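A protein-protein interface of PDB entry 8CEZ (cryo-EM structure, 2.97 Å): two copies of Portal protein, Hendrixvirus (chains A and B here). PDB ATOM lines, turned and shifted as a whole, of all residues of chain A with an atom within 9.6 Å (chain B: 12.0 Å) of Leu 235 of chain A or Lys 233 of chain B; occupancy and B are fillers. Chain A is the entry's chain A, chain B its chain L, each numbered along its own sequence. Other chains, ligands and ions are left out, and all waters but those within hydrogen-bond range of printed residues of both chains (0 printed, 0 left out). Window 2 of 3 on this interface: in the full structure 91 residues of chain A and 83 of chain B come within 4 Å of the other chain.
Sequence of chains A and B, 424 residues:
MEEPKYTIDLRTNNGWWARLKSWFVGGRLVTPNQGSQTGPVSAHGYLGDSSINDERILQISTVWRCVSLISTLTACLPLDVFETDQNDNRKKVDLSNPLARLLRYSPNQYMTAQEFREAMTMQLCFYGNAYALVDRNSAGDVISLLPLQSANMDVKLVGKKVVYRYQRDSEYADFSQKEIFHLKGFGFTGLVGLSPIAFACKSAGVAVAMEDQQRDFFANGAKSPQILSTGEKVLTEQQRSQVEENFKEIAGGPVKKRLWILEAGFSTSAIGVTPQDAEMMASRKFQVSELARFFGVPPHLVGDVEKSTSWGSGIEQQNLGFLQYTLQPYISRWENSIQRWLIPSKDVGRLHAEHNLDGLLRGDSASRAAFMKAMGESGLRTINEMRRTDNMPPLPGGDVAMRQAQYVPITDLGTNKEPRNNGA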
ATOM      1  N   SER A 229     -13.316 -14.212  -6.129  1.00  0.00           N
ATOM      2  CA  SER A 229     -12.581 -14.224  -7.388  1.00  0.00           C
ATOM      3  C   SER A 229     -11.129 -14.656  -7.215  1.00  0.00           C
ATOM      4  O   SER A 229     -10.402 -14.732  -8.215  1.00  0.00           O
ATOM      5  CB  SER A 229     -12.622 -12.841  -8.061  1.00  0.00           C
ATOM      6  OG  SER A 229     -11.662 -11.964  -7.497  1.00  0.00           O
ATOM      7  N   THR A 230     -10.681 -14.941  -5.994  1.00  0.00           N
ATOM      8  CA  THR A 230      -9.346 -15.466  -5.755  1.00  0.00           C
ATOM      9  C   THR A 230      -9.440 -16.521  -4.662  1.00  0.00           C
ATOM     10  O   THR A 230     -10.530 -16.967  -4.295  1.00  0.00           O
ATOM     11  CB  THR A 230      -8.359 -14.353  -5.374  1.00  0.00           C
ATOM     12  OG1 THR A 230      -7.037 -14.897  -5.260  1.00  0.00           O
ATOM     13  CG2 THR A 230      -8.747 -13.713  -4.047  1.00  0.00           C
ATOM     14  N   GLY A 231      -8.280 -16.931  -4.153  1.00  0.00           N
ATOM     15  CA  GLY A 231      -8.212 -17.886  -3.064  1.00  0.00           C
ATOM     16  C   GLY A 231      -7.472 -17.330  -1.863  1.00  0.00           C
ATOM     17  O   GLY A 231      -7.913 -16.356  -1.245  1.00  0.00           O
ATOM     18  N   GLU A 232      -6.355 -17.967  -1.508  1.00  0.00           N
ATOM     19  CA  GLU A 232      -5.438 -17.451  -0.494  1.00  0.00           C
ATOM     20  C   GLU A 232      -4.086 -17.233  -1.170  1.00  0.00           C
ATOM     21  O   GLU A 232      -3.213 -18.100  -1.180  1.00  0.00           O
ATOM     22  CB  GLU A 232      -5.332 -18.408   0.690  1.00  0.00           C
ATOM     23  CG  GLU A 232      -6.429 -18.255   1.719  1.00  0.00           C
ATOM     24  CD  GLU A 232      -6.304 -19.248   2.863  1.00  0.00           C
ATOM     25  OE1 GLU A 232      -5.589 -20.258   2.703  1.00  0.00           O
ATOM     26  OE2 GLU A 232      -6.922 -19.015   3.921  1.00  0.00           O
ATOM     27  N   LYS A 233      -3.917 -16.039  -1.736  1.00  0.00           N
ATOM     28  CA  LYS A 233      -2.695 -15.665  -2.448  1.00  0.00           C
ATOM     29  C   LYS A 233      -2.468 -16.559  -3.670  1.00  0.00           C
ATOM     30  O   LYS A 233      -1.476 -17.283  -3.772  1.00  0.00           O
ATOM     31  CB  LYS A 233      -1.490 -15.710  -1.504  1.00  0.00           C
ATOM     32  CG  LYS A 233      -1.681 -14.911  -0.230  1.00  0.00           C
ATOM     33  CD  LYS A 233      -0.372 -14.306   0.229  1.00  0.00           C
ATOM     34  CE  LYS A 233      -0.581 -13.083   1.092  1.00  0.00           C
ATOM     35  NZ  LYS A 233       0.584 -12.166   0.979  1.00  0.00           N
ATOM     36  N   VAL A 234      -3.413 -16.490  -4.605  1.00  0.00           N
ATOM     37  CA  VAL A 234      -3.296 -17.247  -5.847  1.00  0.00           C
ATOM     38  C   VAL A 234      -2.524 -16.449  -6.894  1.00  0.00           C
ATOM     39  O   VAL A 234      -1.435 -16.847  -7.325  1.00  0.00           O
ATOM     40  CB  VAL A 234      -4.691 -17.644  -6.362  1.00  0.00           C
ATOM     41  CG1 VAL A 234      -4.630 -18.068  -7.825  1.00  0.00           C
ATOM     42  CG2 VAL A 234      -5.267 -18.752  -5.504  1.00  0.00           C
ATOM     43  N   LEU A 235      -3.069 -15.306  -7.308  1.00  0.00           N
ATOM     44  CA  LEU A 235      -2.455 -14.490  -8.350  1.00  0.00           C
ATOM     45  C   LEU A 235      -3.034 -13.084  -8.278  1.00  0.00           C
ATOM     46  O   LEU A 235      -4.257 -12.917  -8.266  1.00  0.00           O
ATOM     47  CB  LEU A 235      -2.701 -15.093  -9.743  1.00  0.00           C
ATOM     48  CG  LEU A 235      -1.778 -16.224 -10.216  1.00  0.00           C
ATOM     49  CD1 LEU A 235      -2.157 -16.670 -11.620  1.00  0.00           C
ATOM     50  CD2 LEU A 235      -0.307 -15.807 -10.163  1.00  0.00           C
ATOM     51  N   THR A 236      -2.155 -12.078  -8.230  1.00  0.00           N
ATOM     52  CA  THR A 236      -2.574 -10.681  -8.202  1.00  0.00           C
ATOM     53  C   THR A 236      -2.061  -9.898  -9.406  1.00  0.00           C
ATOM     54  O   THR A 236      -1.868  -8.682  -9.313  1.00  0.00           O
ATOM     55  CB  THR A 236      -2.120 -10.005  -6.905  1.00  0.00           C
ATOM     56  OG1 THR A 236      -0.688  -9.998  -6.836  1.00  0.00           O
ATOM     57  CG2 THR A 236      -2.689 -10.728  -5.692  1.00  0.00           C
ATOM     58  N   GLU A 237      -1.809 -10.571 -10.534  1.00  0.00           N
ATOM     59  CA  GLU A 237      -1.469  -9.867 -11.763  1.00  0.00           C
ATOM     60  C   GLU A 237      -2.026 -10.510 -13.027  1.00  0.00           C
ATOM     61  O   GLU A 237      -1.720 -10.025 -14.121  1.00  0.00           O
ATOM     62  CB  GLU A 237       0.060  -9.730 -11.892  1.00  0.00           C
ATOM     63  CG  GLU A 237       0.801 -11.043 -12.105  1.00  0.00           C
ATOM     64  CD  GLU A 237       1.077 -11.339 -13.567  1.00  0.00           C
ATOM     65  OE1 GLU A 237       1.201 -10.384 -14.363  1.00  0.00           O
ATOM     66  OE2 GLU A 237       1.182 -12.533 -13.918  1.00  0.00           O
ATOM     67  N   GLN A 238      -2.825 -11.573 -12.927  1.00  0.00           N
ATOM     68  CA  GLN A 238      -3.370 -12.221 -14.112  1.00  0.00           C
ATOM     69  C   GLN A 238      -4.767 -12.754 -13.829  1.00  0.00           C
ATOM     70  O   GLN A 238      -5.001 -13.389 -12.798  1.00  0.00           O
ATOM     71  CB  GLN A 238      -2.472 -13.368 -14.588  1.00  0.00           C
ATOM     72  CG  GLN A 238      -1.508 -12.972 -15.697  1.00  0.00           C
ATOM     73  CD  GLN A 238      -1.024 -14.163 -16.500  1.00  0.00           C
ATOM     74  OE1 GLN A 238      -1.268 -15.314 -16.138  1.00  0.00           O
ATOM     75  NE2 GLN A 238      -0.343 -13.891 -17.606  1.00  0.00           N
ATOM     76  N   GLN A 239      -5.682 -12.500 -14.765  1.00  0.00           N
ATOM     77  CA  GLN A 239      -7.052 -13.011 -14.704  1.00  0.00           C
ATOM     78  C   GLN A 239      -7.692 -12.691 -13.356  1.00  0.00           C
ATOM     79  O   GLN A 239      -8.308 -13.542 -12.710  1.00  0.00           O
ATOM     80  CB  GLN A 239      -7.085 -14.516 -14.981  1.00  0.00           C
ATOM     81  CG  GLN A 239      -6.324 -14.943 -16.230  1.00  0.00           C
ATOM     82  CD  GLN A 239      -6.295 -16.450 -16.412  1.00  0.00           C
ATOM     83  OE1 GLN A 239      -6.729 -17.203 -15.538  1.00  0.00           O
ATOM     84  NE2 GLN A 239      -5.783 -16.897 -17.554  1.00  0.00           N
ATOM     85  N   ARG A 240      -7.538 -11.437 -12.928  1.00  0.00           N
ATOM     86  CA  ARG A 240      -8.004 -11.021 -11.612  1.00  0.00           C
ATOM     87  C   ARG A 240      -8.671  -9.649 -11.606  1.00  0.00           C
ATOM     88  O   ARG A 240      -8.698  -8.998 -10.552  1.00  0.00           O
ATOM     89  CB  ARG A 240      -6.830 -11.049 -10.620  1.00  0.00           C
ATOM     90  CG  ARG A 240      -5.648 -10.156 -11.001  1.00  0.00           C
ATOM     91  CD  ARG A 240      -5.795  -8.738 -10.490  1.00  0.00           C
ATOM     92  NE  ARG A 240      -4.602  -7.938 -10.726  1.00  0.00           N
ATOM     93  CZ  ARG A 240      -4.520  -6.637 -10.488  1.00  0.00           C
ATOM     94  NH1 ARG A 240      -5.550  -5.955 -10.012  1.00  0.00           N
ATOM     95  NH2 ARG A 240      -3.375  -6.004 -10.731  1.00  0.00           N
ATOM     96  N   SER A 241      -9.214  -9.190 -12.729  1.00  0.00           N
ATOM     97  CA  SER A 241      -9.917  -7.914 -12.789  1.00  0.00           C
ATOM     98  C   SER A 241     -11.322  -8.028 -13.355  1.00  0.00           C
ATOM     99  O   SER A 241     -12.235  -7.358 -12.868  1.00  0.00           O
ATOM    100  CB  SER A 241      -9.111  -6.915 -13.633  1.00  0.00           C
ATOM    101  OG  SER A 241      -8.784  -7.464 -14.899  1.00  0.00           O
ATOM    102  N   GLN A 242     -11.516  -8.864 -14.375  1.00  0.00           N
ATOM    103  CA  GLN A 242     -12.802  -8.998 -15.046  1.00  0.00           C
ATOM    104  C   GLN A 242     -13.682 -10.089 -14.455  1.00  0.00           C
ATOM    105  O   GLN A 242     -14.893 -10.080 -14.693  1.00  0.00           O
ATOM    106  CB  GLN A 242     -12.588  -9.281 -16.537  1.00  0.00           C
ATOM    107  CG  GLN A 242     -11.802 -10.561 -16.828  1.00  0.00           C
ATOM    108  CD  GLN A 242     -10.301 -10.318 -16.929  1.00  0.00           C
ATOM    109  OE1 GLN A 242      -9.813  -9.233 -16.610  1.00  0.00           O
ATOM    110  NE2 GLN A 242      -9.561 -11.336 -17.360  1.00  0.00           N
ATOM    111  N   VAL A 243     -13.107 -11.033 -13.710  1.00  0.00           N
ATOM    112  CA  VAL A 243     -13.891 -12.156 -13.210  1.00  0.00           C
ATOM    113  C   VAL A 243     -14.974 -11.668 -12.254  1.00  0.00           C
ATOM    114  O   VAL A 243     -16.110 -12.158 -12.280  1.00  0.00           O
ATOM    115  CB  VAL A 243     -12.965 -13.196 -12.554  1.00  0.00           C
ATOM    116  CG1 VAL A 243     -13.771 -14.279 -11.880  1.00  0.00           C
ATOM    117  CG2 VAL A 243     -12.031 -13.806 -13.596  1.00  0.00           C
ATOM    118  N   ILE A 261     -19.083 -19.730 -10.475  1.00  0.00           N
ATOM    119  CA  ILE A 261     -18.524 -19.893  -9.137  1.00  0.00           C
ATOM    120  C   ILE A 261     -17.221 -20.672  -9.243  1.00  0.00           C
ATOM    121  O   ILE A 261     -17.100 -21.584 -10.069  1.00  0.00           O
ATOM    122  CB  ILE A 261     -19.511 -20.611  -8.191  1.00  0.00           C
ATOM    123  CG1 ILE A 261     -20.914 -19.995  -8.294  1.00  0.00           C
ATOM    124  CG2 ILE A 261     -19.011 -20.535  -6.762  1.00  0.00           C
ATOM    125  CD1 ILE A 261     -22.017 -20.900  -7.799  1.00  0.00           C
ATOM    126  N   LEU A 262     -16.248 -20.317  -8.406  1.00  0.00           N
ATOM    127  CA  LEU A 262     -14.933 -20.940  -8.486  1.00  0.00           C
ATOM    128  C   LEU A 262     -15.008 -22.423  -8.122  1.00  0.00           C
ATOM    129  O   LEU A 262     -15.830 -22.856  -7.311  1.00  0.00           O
ATOM    130  CB  LEU A 262     -13.932 -20.230  -7.571  1.00  0.00           C
ATOM    131  CG  LEU A 262     -13.495 -18.819  -7.977  1.00  0.00           C
ATOM    132  CD1 LEU A 262     -12.412 -18.332  -7.040  1.00  0.00           C
ATOM    133  CD2 LEU A 262     -13.018 -18.754  -9.420  1.00  0.00           C
ATOM    134  N   GLU A 263     -14.107 -23.199  -8.737  1.00  0.00           N
ATOM    135  CA  GLU A 263     -14.170 -24.655  -8.651  1.00  0.00           C
ATOM    136  C   GLU A 263     -14.267 -25.151  -7.217  1.00  0.00           C
ATOM    137  O   GLU A 263     -15.089 -26.026  -6.924  1.00  0.00           O
ATOM    138  CB  GLU A 263     -12.945 -25.272  -9.330  1.00  0.00           C
ATOM    139  CG  GLU A 263     -12.941 -26.797  -9.357  1.00  0.00           C
ATOM    140  CD  GLU A 263     -12.229 -27.410  -8.167  1.00  0.00           C
ATOM    141  OE1 GLU A 263     -11.237 -26.821  -7.688  1.00  0.00           O
ATOM    142  OE2 GLU A 263     -12.668 -28.482  -7.704  1.00  0.00           O
ATOM    143  N   ALA A 264     -13.431 -24.628  -6.317  1.00  0.00           N
ATOM    144  CA  ALA A 264     -13.397 -25.138  -4.950  1.00  0.00           C
ATOM    145  C   ALA A 264     -14.801 -25.244  -4.368  1.00  0.00           C
ATOM    146  O   ALA A 264     -15.222 -26.314  -3.913  1.00  0.00           O
ATOM    147  CB  ALA A 264     -12.519 -24.239  -4.077  1.00  0.00           C
ATOM    148  N   LEU B 228     -21.934 -23.128 -14.392  1.00  0.00           N
ATOM    149  CA  LEU B 228     -20.478 -23.142 -14.359  1.00  0.00           C
ATOM    150  C   LEU B 228     -19.967 -23.782 -15.640  1.00  0.00           C
ATOM    151  O   LEU B 228     -20.416 -24.869 -16.014  1.00  0.00           O
ATOM    152  CB  LEU B 228     -19.937 -23.917 -13.152  1.00  0.00           C
ATOM    153  CG  LEU B 228     -19.744 -23.166 -11.837  1.00  0.00           C
ATOM    154  CD1 LEU B 228     -21.063 -22.987 -11.098  1.00  0.00           C
ATOM    155  CD2 LEU B 228     -18.735 -23.907 -10.973  1.00  0.00           C
ATOM    156  N   SER B 229     -19.012 -23.114 -16.299  1.00  0.00           N
ATOM    157  CA  SER B 229     -18.408 -23.655 -17.512  1.00  0.00           C
ATOM    158  C   SER B 229     -16.897 -23.803 -17.397  1.00  0.00           C
ATOM    159  O   SER B 229     -16.265 -24.279 -18.349  1.00  0.00           O
ATOM    160  CB  SER B 229     -18.740 -22.777 -18.731  1.00  0.00           C
ATOM    161  OG  SER B 229     -17.898 -21.637 -18.792  1.00  0.00           O
ATOM    162  N   THR B 230     -16.297 -23.419 -16.272  1.00  0.00           N
ATOM    163  CA  THR B 230     -14.876 -23.617 -16.038  1.00  0.00           C
ATOM    164  C   THR B 230     -14.681 -24.020 -14.585  1.00  0.00           C
ATOM    165  O   THR B 230     -15.638 -24.334 -13.873  1.00  0.00           O
ATOM    166  CB  THR B 230     -14.063 -22.359 -16.375  1.00  0.00           C
ATOM    167  OG1 THR B 230     -12.670 -22.614 -16.158  1.00  0.00           O
ATOM    168  CG2 THR B 230     -14.497 -21.184 -15.507  1.00  0.00           C
ATOM    169  N   GLY B 231     -13.423 -24.018 -14.151  1.00  0.00           N
ATOM    170  CA  GLY B 231     -13.088 -24.304 -12.770  1.00  0.00           C
ATOM    171  C   GLY B 231     -12.311 -23.179 -12.117  1.00  0.00           C
ATOM    172  O   GLY B 231     -12.813 -22.058 -11.977  1.00  0.00           O
ATOM    173  N   GLU B 232     -11.084 -23.481 -11.689  1.00  0.00           N
ATOM    174  CA  GLU B 232     -10.156 -22.479 -11.168  1.00  0.00           C
ATOM    175  C   GLU B 232      -8.942 -22.448 -12.096  1.00  0.00           C
ATOM    176  O   GLU B 232      -7.953 -23.153 -11.900  1.00  0.00           O
ATOM    177  CB  GLU B 232      -9.761 -22.798  -9.729  1.00  0.00           C
ATOM    178  CG  GLU B 232     -10.693 -22.228  -8.682  1.00  0.00           C
ATOM    179  CD  GLU B 232     -10.333 -22.661  -7.273  1.00  0.00           C
ATOM    180  OE1 GLU B 232      -9.593 -23.655  -7.119  1.00  0.00           O
ATOM    181  OE2 GLU B 232     -10.794 -22.005  -6.317  1.00  0.00           O
ATOM    182  N   LYS B 233      -9.032 -21.607 -13.126  1.00  0.00           N
ATOM    183  CA  LYS B 233      -7.961 -21.445 -14.108  1.00  0.00           C
ATOM    184  C   LYS B 233      -7.683 -22.757 -14.846  1.00  0.00           C
ATOM    185  O   LYS B 233      -6.601 -23.339 -14.755  1.00  0.00           O
ATOM    186  CB  LYS B 233      -6.692 -20.909 -13.439  1.00  0.00           C
ATOM    187  CG  LYS B 233      -6.900 -19.610 -12.685  1.00  0.00           C
ATOM    188  CD  LYS B 233      -5.668 -18.733 -12.759  1.00  0.00           C
ATOM    189  CE  LYS B 233      -5.999 -17.273 -12.536  1.00  0.00           C
ATOM    190  NZ  LYS B 233      -4.991 -16.402 -13.196  1.00  0.00           N
ATOM    191  N   VAL B 234      -8.692 -23.216 -15.584  1.00  0.00           N
ATOM    192  CA  VAL B 234      -8.567 -24.463 -16.334  1.00  0.00           C
ATOM    193  C   VAL B 234      -8.071 -24.194 -17.751  1.00  0.00           C
ATOM    194  O   VAL B 234      -6.983 -24.634 -18.142  1.00  0.00           O
ATOM    195  CB  VAL B 234      -9.911 -25.214 -16.343  1.00  0.00           C
ATOM    196  CG1 VAL B 234      -9.943 -26.250 -17.460  1.00  0.00           C
ATOM    197  CG2 VAL B 234     -10.155 -25.867 -14.998  1.00  0.00           C
ATOM    198  N   LEU B 235      -8.858 -23.461 -18.540  1.00  0.00           N
ATOM    199  CA  LEU B 235      -8.533 -23.223 -19.943  1.00  0.00           C
ATOM    200  C   LEU B 235      -9.327 -22.024 -20.438  1.00  0.00           C
ATOM    201  O   LEU B 235     -10.560 -22.018 -20.352  1.00  0.00           O
ATOM    202  CB  LEU B 235      -8.849 -24.457 -20.802  1.00  0.00           C
ATOM    203  CG  LEU B 235      -7.791 -25.561 -20.905  1.00  0.00           C
ATOM    204  CD1 LEU B 235      -8.281 -26.676 -21.813  1.00  0.00           C
ATOM    205  CD2 LEU B 235      -6.452 -25.018 -21.403  1.00  0.00           C
ATOM    206  N   THR B 236      -8.624 -21.016 -20.959  1.00  0.00           N
ATOM    207  CA  THR B 236      -9.263 -19.824 -21.506  1.00  0.00           C
ATOM    208  C   THR B 236      -9.026 -19.678 -23.006  1.00  0.00           C
ATOM    209  O   THR B 236      -9.091 -18.561 -23.532  1.00  0.00           O
ATOM    210  CB  THR B 236      -8.778 -18.568 -20.776  1.00  0.00           C
ATOM    211  OG1 THR B 236      -7.374 -18.391 -20.999  1.00  0.00           O
ATOM    212  CG2 THR B 236      -9.049 -18.673 -19.280  1.00  0.00           C
ATOM    213  N   GLU B 237      -8.732 -20.775 -23.710  1.00  0.00           N
ATOM    214  CA  GLU B 237      -8.602 -20.716 -25.159  1.00  0.00           C
ATOM    215  C   GLU B 237      -9.147 -21.938 -25.891  1.00  0.00           C
ATOM    216  O   GLU B 237      -9.005 -22.002 -27.116  1.00  0.00           O
ATOM    217  CB  GLU B 237      -7.129 -20.501 -25.551  1.00  0.00           C
ATOM    218  CG  GLU B 237      -6.205 -21.668 -25.227  1.00  0.00           C
ATOM    219  CD  GLU B 237      -6.039 -22.633 -26.388  1.00  0.00           C
ATOM    220  OE1 GLU B 237      -6.201 -22.209 -27.552  1.00  0.00           O
ATOM    221  OE2 GLU B 237      -5.734 -23.817 -26.134  1.00  0.00           O
ATOM    222  N   GLN B 238      -9.758 -22.902 -25.203  1.00  0.00           N
ATOM    223  CA  GLN B 238     -10.298 -24.077 -25.874  1.00  0.00           C
ATOM    224  C   GLN B 238     -11.560 -24.560 -25.174  1.00  0.00           C
ATOM    225  O   GLN B 238     -11.567 -24.757 -23.956  1.00  0.00           O
ATOM    226  CB  GLN B 238      -9.273 -25.217 -25.928  1.00  0.00           C
ATOM    227  CG  GLN B 238      -8.481 -25.271 -27.226  1.00  0.00           C
ATOM    228  CD  GLN B 238      -7.910 -26.647 -27.508  1.00  0.00           C
ATOM    229  OE1 GLN B 238      -7.967 -27.542 -26.663  1.00  0.00           O
ATOM    230  NE2 GLN B 238      -7.368 -26.828 -28.705  1.00  0.00           N
ATOM    231  N   GLN B 239     -12.616 -24.763 -25.962  1.00  0.00           N
ATOM    232  CA  GLN B 239     -13.885 -25.309 -25.478  1.00  0.00           C
ATOM    233  C   GLN B 239     -14.399 -24.515 -24.279  1.00  0.00           C
ATOM    234  O   GLN B 239     -14.734 -25.065 -23.228  1.00  0.00           O
ATOM    235  CB  GLN B 239     -13.744 -26.792 -25.132  1.00  0.00           C
ATOM    236  CG  GLN B 239     -13.082 -27.622 -26.222  1.00  0.00           C
ATOM    237  CD  GLN B 239     -12.839 -29.059 -25.802  1.00  0.00           C
ATOM    238  OE1 GLN B 239     -13.016 -29.418 -24.636  1.00  0.00           O
ATOM    239  NE2 GLN B 239     -12.430 -29.890 -26.754  1.00  0.00           N
ATOM    240  N   ARG B 240     -14.458 -23.193 -24.452  1.00  0.00           N
ATOM    241  CA  ARG B 240     -14.845 -22.294 -23.374  1.00  0.00           C
ATOM    242  C   ARG B 240     -15.760 -21.163 -23.835  1.00  0.00           C
ATOM    243  O   ARG B 240     -15.819 -20.125 -23.160  1.00  0.00           O
ATOM    244  CB  ARG B 240     -13.590 -21.710 -22.705  1.00  0.00           C
ATOM    245  CG  ARG B 240     -12.589 -21.121 -23.695  1.00  0.00           C
ATOM    246  CD  ARG B 240     -12.853 -19.659 -23.974  1.00  0.00           C
ATOM    247  NE  ARG B 240     -11.963 -19.137 -25.002  1.00  0.00           N
ATOM    248  CZ  ARG B 240     -12.075 -17.929 -25.535  1.00  0.00           C
ATOM    249  NH1 ARG B 240     -13.018 -17.085 -25.146  1.00  0.00           N
ATOM    250  NH2 ARG B 240     -11.222 -17.562 -26.489  1.00  0.00           N
ATOM    251  N   LEU B 262     -21.043 -29.705 -14.913  1.00  0.00           N
ATOM    252  CA  LEU B 262     -19.649 -30.128 -14.952  1.00  0.00           C
ATOM    253  C   LEU B 262     -19.371 -31.214 -13.914  1.00  0.00           C
ATOM    254  O   LEU B 262     -19.953 -31.245 -12.825  1.00  0.00           O
ATOM    255  CB  LEU B 262     -18.706 -28.943 -14.732  1.00  0.00           C
ATOM    256  CG  LEU B 262     -18.569 -27.959 -15.898  1.00  0.00           C
ATOM    257  CD1 LEU B 262     -17.487 -26.952 -15.590  1.00  0.00           C
ATOM    258  CD2 LEU B 262     -18.282 -28.667 -17.215  1.00  0.00           C
ATOM    259  N   ALA B 264     -17.196 -32.098 -11.682  1.00  0.00           N
ATOM    260  CA  ALA B 264     -16.895 -31.853 -10.274  1.00  0.00           C
ATOM    261  C   ALA B 264     -18.162 -31.892  -9.429  1.00  0.00           C
ATOM    262  O   ALA B 264     -18.252 -32.645  -8.452  1.00  0.00           O
ATOM    263  CB  ALA B 264     -16.185 -30.506 -10.116  1.00  0.00           C
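O of Gln 238 of chain A lies within hydrogen-bond range of NZ of Lys 233 of chain B, 3.0 Å away.
The side-chain amino group (NZ) of Lys 233 of chain B lies within hydrogen-bond range of the side-chain amide oxygen (OE1) of Gln 239 of chain A, at 3.0 Å.
Lys 233 of chain B touches Leu 235 of chain A (NZ to CD1, 3.3 Å).
Ile 261 of chain A touches Leu 228 of chain B (O to CD2, 3.0 Å).
Leu 262 of chain A touches Glu 232 of chain B.
Gly 231 of chain B touches Glu 263 of chain A.
Glu 232 of chain B touches Glu 263 of chain A.
Ala 264 of chain A touches Glu 232 of chain B (CB to OE2, 3.6 Å).
Thr 230 of chain A touches none of the printed residues of chain B.
No residue of chain B comes within 4 Å of Gly 231 of chain A.
No residue of chain B comes within 4 Å of Val 234 of chain A.
Of the printed residues of chain B, Leu 235 of chain A touches Lys 233 (3.3 Å).
No residue of chain B comes within 4 Å of Thr 236 of chain A.
Glu 237 of chain A touches none of the printed residues of chain B.
Gln 238 of chain A touches one residue of chain B.
Of chain B, only Lys 233 (3.0 Å) comes within 4 Å of Gln 239 of chain A.
No residue of chain B comes within 4 Å of Arg 240 of chain A.
Printed residues of chain B within 4 Å of Leu 262 of chain A: Glu 232 (3.8 Å).
Of the printed residues of chain A, Leu 228 of chain B touches Ile 261 (3.0 Å).
Of chain A, only Leu 235, Gln 238 and Gln 239 come within 4 Å of Lys 233 of chain B.
Val 234 of chain B touches none of the printed residues of chain A.
Leu 235 of chain B touches none of the printed residues of chain A.
The nearest printed residue of chain A that does not touch Leu 228 of chain B is Leu 262 of chain A (4.8 Å).
Hydrophobic or aromatic side chains of chain B that line the printed part of chain A: Leu 228.
Hydrophobic or aromatic side chains of chain A within 4 Å of the printed part of chain B: Leu 235, Leu 262 and Ala 264.
Along chain A the printed residues that touch a printed residue of chain B span positions 235 to 264.
Among the printed residues, 8 pairs touch across the chains.
Among the printed residues, no Asp or Glu carboxylate lies within 4 Å of a Lys or Arg side-chain nitrogen of the other chain.
Gln 238 of chain A touches Lys 233 of chain B, but with the chains exchanged Lys 233 of chain A does not touch Gln 238 of chain B (23.6 Å).
Gln 239 of chain A touches Lys 233 of chain B, but with the chains exchanged Lys 233 of chain A does not touch Gln 239 of chain B (24.6 Å).
Leu 262 of chain A touches Glu 232 of chain B, but with the chains exchanged Glu 232 of chain A does not touch Leu 262 of chain B (20.1 Å).
Ala 264 of chain A touches Glu 232 of chain B, but with the chains exchanged Glu 232 of chain A does not touch Ala 264 of chain B (18.1 Å).
Of the 8 pairs that touch across the chains among the printed residues, none has its exchanged pair printed and touching as well.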
